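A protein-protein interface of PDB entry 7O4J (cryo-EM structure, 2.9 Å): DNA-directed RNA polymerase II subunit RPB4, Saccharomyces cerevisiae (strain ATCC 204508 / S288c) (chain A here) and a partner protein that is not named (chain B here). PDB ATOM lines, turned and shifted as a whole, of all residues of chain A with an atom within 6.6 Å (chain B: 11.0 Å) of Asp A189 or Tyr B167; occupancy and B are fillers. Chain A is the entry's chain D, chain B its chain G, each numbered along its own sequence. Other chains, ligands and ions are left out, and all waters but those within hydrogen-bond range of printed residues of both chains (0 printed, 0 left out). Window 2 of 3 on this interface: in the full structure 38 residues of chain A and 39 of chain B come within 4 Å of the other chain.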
ATOM      1  N   ASP A 186       5.035  25.535  22.195  1.00  0.00           N
ATOM      2  CA  ASP A 186       5.866  24.361  22.433  1.00  0.00           C
ATOM      3  C   ASP A 186       6.905  24.125  21.347  1.00  0.00           C
ATOM      4  O   ASP A 186       7.996  23.632  21.650  1.00  0.00           O
ATOM      5  CB  ASP A 186       4.988  23.111  22.557  1.00  0.00           C
ATOM      6  CG  ASP A 186       4.490  22.887  23.971  1.00  0.00           C
ATOM      7  OD1 ASP A 186       5.330  22.687  24.874  1.00  0.00           O
ATOM      8  OD2 ASP A 186       3.259  22.911  24.180  1.00  0.00           O
ATOM      9  N   THR A 187       6.599  24.462  20.098  1.00  0.00           N
ATOM     10  CA  THR A 187       7.503  24.244  18.979  1.00  0.00           C
ATOM     11  C   THR A 187       7.758  25.559  18.254  1.00  0.00           C
ATOM     12  O   THR A 187       6.943  26.483  18.290  1.00  0.00           O
ATOM     13  CB  THR A 187       6.935  23.215  17.992  1.00  0.00           C
ATOM     14  OG1 THR A 187       5.911  23.824  17.197  1.00  0.00           O
ATOM     15  CG2 THR A 187       6.353  22.021  18.737  1.00  0.00           C
ATOM     16  N   ALA A 188       8.914  25.629  17.589  1.00  0.00           N
ATOM     17  CA  ALA A 188       9.256  26.832  16.839  1.00  0.00           C
ATOM     18  C   ALA A 188       8.224  27.128  15.759  1.00  0.00           C
ATOM     19  O   ALA A 188       7.983  28.295  15.434  1.00  0.00           O
ATOM     20  CB  ALA A 188      10.645  26.688  16.219  1.00  0.00           C
ATOM     21  N   ASP A 189       7.605  26.089  15.194  1.00  0.00           N
ATOM     22  CA  ASP A 189       6.572  26.308  14.189  1.00  0.00           C
ATOM     23  C   ASP A 189       5.377  27.054  14.768  1.00  0.00           C
ATOM     24  O   ASP A 189       4.815  27.932  14.103  1.00  0.00           O
ATOM     25  CB  ASP A 189       6.124  24.971  13.598  1.00  0.00           C
ATOM     26  CG  ASP A 189       5.098  25.135  12.495  1.00  0.00           C
ATOM     27  OD1 ASP A 189       5.217  26.100  11.710  1.00  0.00           O
ATOM     28  OD2 ASP A 189       4.174  24.300  12.413  1.00  0.00           O
ATOM     29  N   GLU A 190       4.975  26.720  15.996  1.00  0.00           N
ATOM     30  CA  GLU A 190       3.839  27.400  16.611  1.00  0.00           C
ATOM     31  C   GLU A 190       4.106  28.891  16.771  1.00  0.00           C
ATOM     32  O   GLU A 190       3.235  29.718  16.477  1.00  0.00           O
ATOM     33  CB  GLU A 190       3.525  26.766  17.965  1.00  0.00           C
ATOM     34  CG  GLU A 190       2.257  27.288  18.616  1.00  0.00           C
ATOM     35  CD  GLU A 190       1.872  26.502  19.854  1.00  0.00           C
ATOM     36  OE1 GLU A 190       2.629  25.587  20.237  1.00  0.00           O
ATOM     37  OE2 GLU A 190       0.811  26.800  20.443  1.00  0.00           O
ATOM     38  N   ALA A 191       5.304  29.255  17.231  1.00  0.00           N
ATOM     39  CA  ALA A 191       5.638  30.663  17.393  1.00  0.00           C
ATOM     40  C   ALA A 191       5.821  31.370  16.059  1.00  0.00           C
ATOM     41  O   ALA A 191       5.639  32.590  15.989  1.00  0.00           O
ATOM     42  CB  ALA A 191       6.906  30.808  18.234  1.00  0.00           C
ATOM     43  N   LYS A 192       6.176  30.637  15.002  1.00  0.00           N
ATOM     44  CA  LYS A 192       6.348  31.253  13.692  1.00  0.00           C
ATOM     45  C   LYS A 192       5.013  31.591  13.039  1.00  0.00           C
ATOM     46  O   LYS A 192       4.945  32.526  12.233  1.00  0.00           O
ATOM     47  CB  LYS A 192       7.157  30.329  12.782  1.00  0.00           C
ATOM     48  CG  LYS A 192       8.615  30.178  13.192  1.00  0.00           C
ATOM     49  CD  LYS A 192       9.463  31.329  12.677  1.00  0.00           C
ATOM     50  CE  LYS A 192      10.930  31.138  13.027  1.00  0.00           C
ATOM     51  NZ  LYS A 192      11.600  30.174  12.112  1.00  0.00           N
ATOM     52  N   THR A 193       3.954  30.853  13.368  1.00  0.00           N
ATOM     53  CA  THR A 193       2.629  31.120  12.821  1.00  0.00           C
ATOM     54  C   THR A 193       1.766  31.977  13.734  1.00  0.00           C
ATOM     55  O   THR A 193       0.982  32.793  13.237  1.00  0.00           O
ATOM     56  CB  THR A 193       1.895  29.803  12.529  1.00  0.00           C
ATOM     57  OG1 THR A 193       0.644  30.083  11.888  1.00  0.00           O
ATOM     58  CG2 THR A 193       1.641  29.018  13.811  1.00  0.00           C
ATOM     59  N   LEU A 194       1.886  31.816  15.053  1.00  0.00           N
ATOM     60  CA  LEU A 194       1.168  32.689  15.973  1.00  0.00           C
ATOM     61  C   LEU A 194       1.754  34.093  15.983  1.00  0.00           C
ATOM     62  O   LEU A 194       1.048  35.054  16.309  1.00  0.00           O
ATOM     63  CB  LEU A 194       1.197  32.105  17.387  1.00  0.00           C
ATOM     64  CG  LEU A 194       0.363  30.848  17.653  1.00  0.00           C
ATOM     65  CD1 LEU A 194       0.244  30.614  19.148  1.00  0.00           C
ATOM     66  CD2 LEU A 194      -1.017  30.939  17.020  1.00  0.00           C
ATOM     67  N   ASP A 204      15.248  28.723  13.776  1.00  0.00           N
ATOM     68  CA  ASP A 204      14.531  27.739  14.578  1.00  0.00           C
ATOM     69  C   ASP A 204      15.405  27.184  15.693  1.00  0.00           C
ATOM     70  O   ASP A 204      14.892  26.754  16.732  1.00  0.00           O
ATOM     71  CB  ASP A 204      14.028  26.601  13.687  1.00  0.00           C
ATOM     72  CG  ASP A 204      13.296  27.102  12.458  1.00  0.00           C
ATOM     73  OD1 ASP A 204      12.654  28.170  12.541  1.00  0.00           O
ATOM     74  OD2 ASP A 204      13.363  26.428  11.409  1.00  0.00           O
ATOM     75  N   LEU A 207      15.000  29.715  18.533  1.00  0.00           N
ATOM     76  CA  LEU A 207      13.624  29.745  19.016  1.00  0.00           C
ATOM     77  C   LEU A 207      13.289  28.490  19.812  1.00  0.00           C
ATOM     78  O   LEU A 207      12.604  28.563  20.838  1.00  0.00           O
ATOM     79  CB  LEU A 207      12.662  29.907  17.839  1.00  0.00           C
ATOM     80  CG  LEU A 207      11.243  30.386  18.161  1.00  0.00           C
ATOM     81  CD1 LEU A 207      11.257  31.723  18.891  1.00  0.00           C
ATOM     82  CD2 LEU A 207      10.424  30.481  16.885  1.00  0.00           C
ATOM     83  N   GLU A 208      13.762  27.328  19.355  1.00  0.00           N
ATOM     84  CA  GLU A 208      13.467  26.085  20.060  1.00  0.00           C
ATOM     85  C   GLU A 208      14.018  26.113  21.479  1.00  0.00           C
ATOM     86  O   GLU A 208      13.331  25.708  22.425  1.00  0.00           O
ATOM     87  CB  GLU A 208      14.039  24.897  19.289  1.00  0.00           C
ATOM     88  CG  GLU A 208      13.089  24.308  18.259  1.00  0.00           C
ATOM     89  CD  GLU A 208      12.156  23.270  18.852  1.00  0.00           C
ATOM     90  OE1 GLU A 208      12.637  22.174  19.211  1.00  0.00           O
ATOM     91  OE2 GLU A 208      10.944  23.550  18.961  1.00  0.00           O
ATOM     92  N   LEU A 211      12.095  28.833  23.706  1.00  0.00           N
ATOM     93  CA  LEU A 211      10.808  28.335  24.177  1.00  0.00           C
ATOM     94  C   LEU A 211      10.991  27.328  25.304  1.00  0.00           C
ATOM     95  O   LEU A 211      10.225  27.325  26.274  1.00  0.00           O
ATOM     96  CB  LEU A 211      10.034  27.705  23.018  1.00  0.00           C
ATOM     97  CG  LEU A 211       9.522  28.664  21.942  1.00  0.00           C
ATOM     98  CD1 LEU A 211       8.910  27.883  20.791  1.00  0.00           C
ATOM     99  CD2 LEU A 211       8.512  29.643  22.519  1.00  0.00           C
ATOM    100  N   GLU B  85      -2.789  40.212  15.657  1.00  0.00           N
ATOM    101  CA  GLU B  85      -2.233  39.788  16.931  1.00  0.00           C
ATOM    102  C   GLU B  85      -3.062  38.649  17.509  1.00  0.00           C
ATOM    103  O   GLU B  85      -4.280  38.585  17.324  1.00  0.00           O
ATOM    104  CB  GLU B  85      -2.190  40.957  17.917  1.00  0.00           C
ATOM    105  CG  GLU B  85      -1.522  40.628  19.242  1.00  0.00           C
ATOM    106  CD  GLU B  85      -1.486  41.812  20.187  1.00  0.00           C
ATOM    107  OE1 GLU B  85      -1.991  42.891  19.810  1.00  0.00           O
ATOM    108  OE2 GLU B  85      -0.955  41.663  21.306  1.00  0.00           O
ATOM    109  N   VAL B  86      -2.387  37.747  18.217  1.00  0.00           N
ATOM    110  CA  VAL B  86      -3.010  36.572  18.813  1.00  0.00           C
ATOM    111  C   VAL B  86      -3.108  36.796  20.314  1.00  0.00           C
ATOM    112  O   VAL B  86      -2.118  37.154  20.962  1.00  0.00           O
ATOM    113  CB  VAL B  86      -2.217  35.293  18.494  1.00  0.00           C
ATOM    114  CG1 VAL B  86      -2.590  34.173  19.457  1.00  0.00           C
ATOM    115  CG2 VAL B  86      -2.458  34.870  17.055  1.00  0.00           C
ATOM    116  N   VAL B  87      -4.304  36.588  20.864  1.00  0.00           N
ATOM    117  CA  VAL B  87      -4.573  36.802  22.278  1.00  0.00           C
ATOM    118  C   VAL B  87      -5.340  35.603  22.819  1.00  0.00           C
ATOM    119  O   VAL B  87      -5.912  34.809  22.071  1.00  0.00           O
ATOM    120  CB  VAL B  87      -5.363  38.102  22.531  1.00  0.00           C
ATOM    121  CG1 VAL B  87      -4.544  39.311  22.113  1.00  0.00           C
ATOM    122  CG2 VAL B  87      -6.693  38.068  21.794  1.00  0.00           C
ATOM    123  N   ASP B  88      -5.343  35.483  24.143  1.00  0.00           N
ATOM    124  CA  ASP B  88      -6.097  34.460  24.848  1.00  0.00           C
ATOM    125  C   ASP B  88      -7.190  35.125  25.670  1.00  0.00           C
ATOM    126  O   ASP B  88      -7.023  36.244  26.164  1.00  0.00           O
ATOM    127  CB  ASP B  88      -5.192  33.628  25.763  1.00  0.00           C
ATOM    128  CG  ASP B  88      -4.088  32.921  25.003  1.00  0.00           C
ATOM    129  OD1 ASP B  88      -4.159  32.870  23.758  1.00  0.00           O
ATOM    130  OD2 ASP B  88      -3.148  32.416  25.652  1.00  0.00           O
ATOM    131  N   GLY B  89      -8.317  34.435  25.806  1.00  0.00           N
ATOM    132  CA  GLY B  89      -9.429  34.996  26.548  1.00  0.00           C
ATOM    133  C   GLY B  89     -10.438  33.926  26.897  1.00  0.00           C
ATOM    134  O   GLY B  89     -10.285  32.753  26.547  1.00  0.00           O
ATOM    135  N   PRO B 116     -13.806  27.418  12.058  1.00  0.00           N
ATOM    136  CA  PRO B 116     -13.637  26.244  11.199  1.00  0.00           C
ATOM    137  C   PRO B 116     -14.976  25.623  10.830  1.00  0.00           C
ATOM    138  O   PRO B 116     -15.976  25.746  11.540  1.00  0.00           O
ATOM    139  CB  PRO B 116     -12.794  25.291  12.052  1.00  0.00           C
ATOM    140  CG  PRO B 116     -13.063  25.679  13.451  1.00  0.00           C
ATOM    141  CD  PRO B 116     -13.435  27.137  13.455  1.00  0.00           C
ATOM    142  N   GLU B 134     -13.710  17.344  18.122  1.00  0.00           N
ATOM    143  CA  GLU B 134     -12.530  17.399  18.978  1.00  0.00           C
ATOM    144  C   GLU B 134     -12.750  18.222  20.247  1.00  0.00           C
ATOM    145  O   GLU B 134     -12.219  17.874  21.306  1.00  0.00           O
ATOM    146  CB  GLU B 134     -11.334  17.944  18.183  1.00  0.00           C
ATOM    147  CG  GLU B 134     -11.419  19.411  17.770  1.00  0.00           C
ATOM    148  CD  GLU B 134     -12.197  19.615  16.484  1.00  0.00           C
ATOM    149  OE1 GLU B 134     -12.920  18.685  16.069  1.00  0.00           O
ATOM    150  OE2 GLU B 134     -12.082  20.706  15.886  1.00  0.00           O
ATOM    151  N   ASP B 135     -13.518  19.307  20.169  1.00  0.00           N
ATOM    152  CA  ASP B 135     -13.666  20.209  21.303  1.00  0.00           C
ATOM    153  C   ASP B 135     -15.044  20.854  21.289  1.00  0.00           C
ATOM    154  O   ASP B 135     -15.742  20.866  20.273  1.00  0.00           O
ATOM    155  CB  ASP B 135     -12.584  21.298  21.299  1.00  0.00           C
ATOM    156  CG  ASP B 135     -12.508  22.040  19.979  1.00  0.00           C
ATOM    157  OD1 ASP B 135     -13.336  21.757  19.086  1.00  0.00           O
ATOM    158  OD2 ASP B 135     -11.619  22.905  19.832  1.00  0.00           O
ATOM    159  N   ARG B 142     -11.847  28.691  27.352  1.00  0.00           N
ATOM    160  CA  ARG B 142     -10.662  29.471  27.018  1.00  0.00           C
ATOM    161  C   ARG B 142     -10.329  29.254  25.549  1.00  0.00           C
ATOM    162  O   ARG B 142     -10.149  28.112  25.113  1.00  0.00           O
ATOM    163  CB  ARG B 142      -9.485  29.077  27.908  1.00  0.00           C
ATOM    164  CG  ARG B 142      -9.592  29.619  29.327  1.00  0.00           C
ATOM    165  CD  ARG B 142      -8.832  28.762  30.328  1.00  0.00           C
ATOM    166  NE  ARG B 142      -7.435  29.174  30.453  1.00  0.00           N
ATOM    167  CZ  ARG B 142      -6.959  29.964  31.413  1.00  0.00           C
ATOM    168  NH1 ARG B 142      -7.760  30.451  32.353  1.00  0.00           N
ATOM    169  NH2 ARG B 142      -5.670  30.274  31.431  1.00  0.00           N
ATOM    170  N   ILE B 143     -10.240  30.347  24.794  1.00  0.00           N
ATOM    171  CA  ILE B 143     -10.036  30.306  23.353  1.00  0.00           C
ATOM    172  C   ILE B 143      -8.866  31.209  22.993  1.00  0.00           C
ATOM    173  O   ILE B 143      -8.768  32.341  23.479  1.00  0.00           O
ATOM    174  CB  ILE B 143     -11.302  30.742  22.585  1.00  0.00           C
ATOM    175  CG1 ILE B 143     -12.541  30.011  23.112  1.00  0.00           C
ATOM    176  CG2 ILE B 143     -11.133  30.491  21.095  1.00  0.00           C
ATOM    177  CD1 ILE B 143     -12.501  28.506  22.929  1.00  0.00           C
ATOM    178  N   ARG B 144      -7.978  30.706  22.139  1.00  0.00           N
ATOM    179  CA  ARG B 144      -6.898  31.495  21.564  1.00  0.00           C
ATOM    180  C   ARG B 144      -7.387  32.078  20.245  1.00  0.00           C
ATOM    181  O   ARG B 144      -7.673  31.332  19.302  1.00  0.00           O
ATOM    182  CB  ARG B 144      -5.648  30.640  21.355  1.00  0.00           C
ATOM    183  CG  ARG B 144      -4.425  31.429  20.915  1.00  0.00           C
ATOM    184  CD  ARG B 144      -3.141  30.643  21.127  1.00  0.00           C
ATOM    185  NE  ARG B 144      -2.930  30.301  22.532  1.00  0.00           N
ATOM    186  CZ  ARG B 144      -1.749  29.997  23.062  1.00  0.00           C
ATOM    187  NH1 ARG B 144      -0.656  29.988  22.310  1.00  0.00           N
ATOM    188  NH2 ARG B 144      -1.660  29.701  24.350  1.00  0.00           N
ATOM    189  N   VAL B 145      -7.481  33.403  20.179  1.00  0.00           N
ATOM    190  CA  VAL B 145      -8.124  34.097  19.072  1.00  0.00           C
ATOM    191  C   VAL B 145      -7.125  35.041  18.419  1.00  0.00           C
ATOM    192  O   VAL B 145      -6.352  35.717  19.106  1.00  0.00           O
ATOM    193  CB  VAL B 145      -9.370  34.871  19.546  1.00  0.00           C
ATOM    194  CG1 VAL B 145      -9.973  35.657  18.400  1.00  0.00           C
ATOM    195  CG2 VAL B 145     -10.391  33.917  20.137  1.00  0.00           C
ATOM    196  N   LYS B 146      -7.147  35.082  17.091  1.00  0.00           N
ATOM    197  CA  LYS B 146      -6.335  36.005  16.309  1.00  0.00           C
ATOM    198  C   LYS B 146      -7.225  37.147  15.836  1.00  0.00           C
ATOM    199  O   LYS B 146      -8.184  36.923  15.090  1.00  0.00           O
ATOM    200  CB  LYS B 146      -5.696  35.289  15.119  1.00  0.00           C
ATOM    201  CG  LYS B 146      -4.746  36.149  14.304  1.00  0.00           C
ATOM    202  CD  LYS B 146      -4.389  35.474  12.991  1.00  0.00           C
ATOM    203  CE  LYS B 146      -3.411  36.309  12.182  1.00  0.00           C
ATOM    204  NZ  LYS B 146      -3.009  35.629  10.921  1.00  0.00           N
ATOM    205  N   SER B 162     -10.548  35.418  14.859  1.00  0.00           N
ATOM    206  CA  SER B 162     -10.708  34.170  14.130  1.00  0.00           C
ATOM    207  C   SER B 162     -10.002  33.045  14.871  1.00  0.00           C
ATOM    208  O   SER B 162      -9.043  33.267  15.615  1.00  0.00           O
ATOM    209  CB  SER B 162     -10.152  34.281  12.707  1.00  0.00           C
ATOM    210  OG  SER B 162      -8.781  34.634  12.721  1.00  0.00           O
ATOM    211  N   ILE B 163     -10.494  31.827  14.658  1.00  0.00           N
ATOM    212  CA  ILE B 163      -9.889  30.633  15.235  1.00  0.00           C
ATOM    213  C   ILE B 163      -9.689  29.584  14.148  1.00  0.00           C
ATOM    214  O   ILE B 163      -9.531  28.393  14.440  1.00  0.00           O
ATOM    215  CB  ILE B 163     -10.747  30.085  16.392  1.00  0.00           C
ATOM    216  CG1 ILE B 163     -12.136  29.690  15.891  1.00  0.00           C
ATOM    217  CG2 ILE B 163     -10.859  31.120  17.499  1.00  0.00           C
ATOM    218  CD1 ILE B 163     -13.021  29.075  16.954  1.00  0.00           C
ATOM    219  N   LYS B 164      -9.697  30.017  12.885  1.00  0.00           N
ATOM    220  CA  LYS B 164      -9.536  29.085  11.772  1.00  0.00           C
ATOM    221  C   LYS B 164      -8.094  28.609  11.634  1.00  0.00           C
ATOM    222  O   LYS B 164      -7.854  27.437  11.323  1.00  0.00           O
ATOM    223  CB  LYS B 164      -9.998  29.739  10.470  1.00  0.00           C
ATOM    224  CG  LYS B 164     -11.506  29.804  10.310  1.00  0.00           C
ATOM    225  CD  LYS B 164     -11.905  30.630   9.095  1.00  0.00           C
ATOM    226  CE  LYS B 164     -11.727  29.852   7.801  1.00  0.00           C
ATOM    227  NZ  LYS B 164     -12.690  28.722   7.686  1.00  0.00           N
ATOM    228  N   GLU B 165      -7.128  29.496  11.854  1.00  0.00           N
ATOM    229  CA  GLU B 165      -5.734  29.145  11.642  1.00  0.00           C
ATOM    230  C   GLU B 165      -5.290  28.088  12.652  1.00  0.00           C
ATOM    231  O   GLU B 165      -5.932  27.853  13.679  1.00  0.00           O
ATOM    232  CB  GLU B 165      -4.851  30.388  11.744  1.00  0.00           C
ATOM    233  CG  GLU B 165      -3.424  30.179  11.260  1.00  0.00           C
ATOM    234  CD  GLU B 165      -2.846  31.409  10.587  1.00  0.00           C
ATOM    235  OE1 GLU B 165      -3.383  32.517  10.799  1.00  0.00           O
ATOM    236  OE2 GLU B 165      -1.853  31.267   9.843  1.00  0.00           O
ATOM    237  N   ASP B 166      -4.170  27.441  12.343  1.00  0.00           N
ATOM    238  CA  ASP B 166      -3.648  26.390  13.200  1.00  0.00           C
ATOM    239  C   ASP B 166      -3.202  26.963  14.543  1.00  0.00           C
ATOM    240  O   ASP B 166      -2.852  28.140  14.666  1.00  0.00           O
ATOM    241  CB  ASP B 166      -2.476  25.680  12.524  1.00  0.00           C
ATOM    242  CG  ASP B 166      -2.926  24.661  11.497  1.00  0.00           C
ATOM    243  OD1 ASP B 166      -3.908  23.935  11.764  1.00  0.00           O
ATOM    244  OD2 ASP B 166      -2.297  24.584  10.421  1.00  0.00           O
ATOM    245  N   TYR B 167      -3.225  26.105  15.561  1.00  0.00           N
ATOM    246  CA  TYR B 167      -2.812  26.455  16.916  1.00  0.00           C
ATOM    247  C   TYR B 167      -3.724  27.503  17.545  1.00  0.00           C
ATOM    248  O   TYR B 167      -3.339  28.162  18.515  1.00  0.00           O
ATOM    249  CB  TYR B 167      -1.358  26.939  16.940  1.00  0.00           C
ATOM    250  CG  TYR B 167      -0.371  25.902  16.455  1.00  0.00           C
ATOM    251  CD1 TYR B 167      -0.114  24.759  17.200  1.00  0.00           C
ATOM    252  CD2 TYR B 167       0.302  26.064  15.253  1.00  0.00           C
ATOM    253  CE1 TYR B 167       0.786  23.809  16.763  1.00  0.00           C
ATOM    254  CE2 TYR B 167       1.204  25.118  14.806  1.00  0.00           C
ATOM    255  CZ  TYR B 167       1.443  23.992  15.565  1.00  0.00           C
ATOM    256  OH  TYR B 167       2.340  23.047  15.125  1.00  0.00           O
ATOM    257  N   LEU B 168      -4.928  27.669  17.010  1.00  0.00           N
ATOM    258  CA  LEU B 168      -5.932  28.572  17.551  1.00  0.00           C
ATOM    259  C   LEU B 168      -7.094  27.760  18.113  1.00  0.00           C
ATOM    260  O   LEU B 168      -7.148  26.534  17.988  1.00  0.00           O
ATOM    261  CB  LEU B 168      -6.417  29.546  16.474  1.00  0.00           C
ATOM    262  CG  LEU B 168      -5.454  30.653  16.040  1.00  0.00           C
ATOM    263  CD1 LEU B 168      -6.121  31.549  15.009  1.00  0.00           C
ATOM    264  CD2 LEU B 168      -4.979  31.472  17.228  1.00  0.00           C
ATOM    265  N   GLY B 169      -8.034  28.461  18.741  1.00  0.00           N
ATOM    266  CA  GLY B 169      -9.224  27.823  19.267  1.00  0.00           C
ATOM    267  C   GLY B 169      -9.100  27.424  20.722  1.00  0.00           C
ATOM    268  O   GLY B 169      -8.446  28.112  21.510  1.00  0.00           O
ATOM    269  N   ALA B 170      -9.728  26.309  21.088  1.00  0.00           N
ATOM    270  CA  ALA B 170      -9.720  25.860  22.474  1.00  0.00           C
ATOM    271  C   ALA B 170      -8.295  25.592  22.939  1.00  0.00           C
ATOM    272  O   ALA B 170      -7.500  24.977  22.221  1.00  0.00           O
ATOM    273  CB  ALA B 170     -10.572  24.603  22.626  1.00  0.00           C
ATOM    274  N   ILE B 171      -7.975  26.055  24.143  1.00  0.00           N
ATOM    275  CA  ILE B 171      -6.653  25.853  24.719  1.00  0.00           C
ATOM    276  C   ILE B 171      -6.655  24.592  25.575  1.00  0.00           C
ATOM    277  O   ILE B 171      -7.635  24.289  26.254  1.00  0.00           O
ATOM    278  CB  ILE B 171      -6.213  27.076  25.543  1.00  0.00           C
ATOM    279  CG1 ILE B 171      -5.976  28.275  24.620  1.00  0.00           C
ATOM    280  CG2 ILE B 171      -4.956  26.751  26.346  1.00  0.00           C
ATOM    281  CD1 ILE B 171      -5.741  29.582  25.351  1.00  0.00           C
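OE2 of Glu A190 is in salt-bridge range of NH1 of Arg B144, at 3.98 Å. The side-chain hydroxyl (OG1) of Thr A193 is in hydrogen-bond range of the side-chain carboxylate (OE2) of Glu B165, 3.4 Å away.
Ala A188 touches none of the printed residues of chain B. Asp A189 touches just one residue of chain B: Tyr B167. No residue of chain B comes within 4 Å of Lys A192. Of chain B, only Glu B165 and Tyr B167 come within 4 Å of Thr A193. Of the printed residues of chain B, Leu A194 touches Val B86 (3.6 Å), Arg B144 (3.3 Å) and Tyr B167 (3.9 Å). Glu B134 touches none of the printed residues of chain A. Of the printed residues of chain A, Glu B165 touches Thr A193. Asp B166 touches none of the printed residues of chain A. Tyr B167 touches just these residues of chain A: Asp A189, Glu A190, Thr A193 and Leu A194. The nearest residue of chain B that does not touch Asp A189 is Asp B166 (6.8 Å). The nearest residue of chain A that does not touch Tyr B167 is Thr A187 (4.2 Å). The nearest printed residue of chain A that does not touch Arg B144 is Asp A186 (7.2 Å).
Of the 13 printed residues of chain A, 4 touch a printed residue of chain B. Printed residues of chain A that touch a printed residue of chain B: Asp A189, Glu A190, Thr A193 and Leu A194. Among the printed residues, 8 pairs touch across the chains. Among the printed residues, Asp or Glu carboxylates within 4 Å of a Lys or Arg side-chain nitrogen of the other chain: Glu A190 with Arg B144 (3.98 Å).
Tyr B167 touches Asp A189. CG of Glu A190 touches CG of Tyr B167 (3.7 Å). Tyr B167 touches Thr A193 (CD2 to CG2, 3.5 Å). Leu A194 touches Val B86 (O to CG2, 3.6 Å). Leu A194 touches Arg B144. O of Tyr B167 touches CD2 of Leu A194, 3.9 Å away.
The side-chain carboxylate (OE1) of Glu A190 is in hydrogen-bond range of the backbone NH (N) of Asp A186 (3.1 Å). The backbone NH of Asp A189 sits close to the side-chain hydroxyl of Thr A187 (3.5 Å). OG1 of Thr A187 sits at hydrogen-bond distance from N of Glu A190 (3.3 Å). NE of Arg B144 lies within salt-bridge range of OD1 of Asp B88, at 3.1 Å. O of Gly B169 lies within hydrogen-bond range of N of Arg B144 (2.7 Å). The side-chain carboxylate (OE1) of Glu B165 is in salt-bridge range of the side-chain amino group (NZ) of Lys B146 (3.1 Å).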
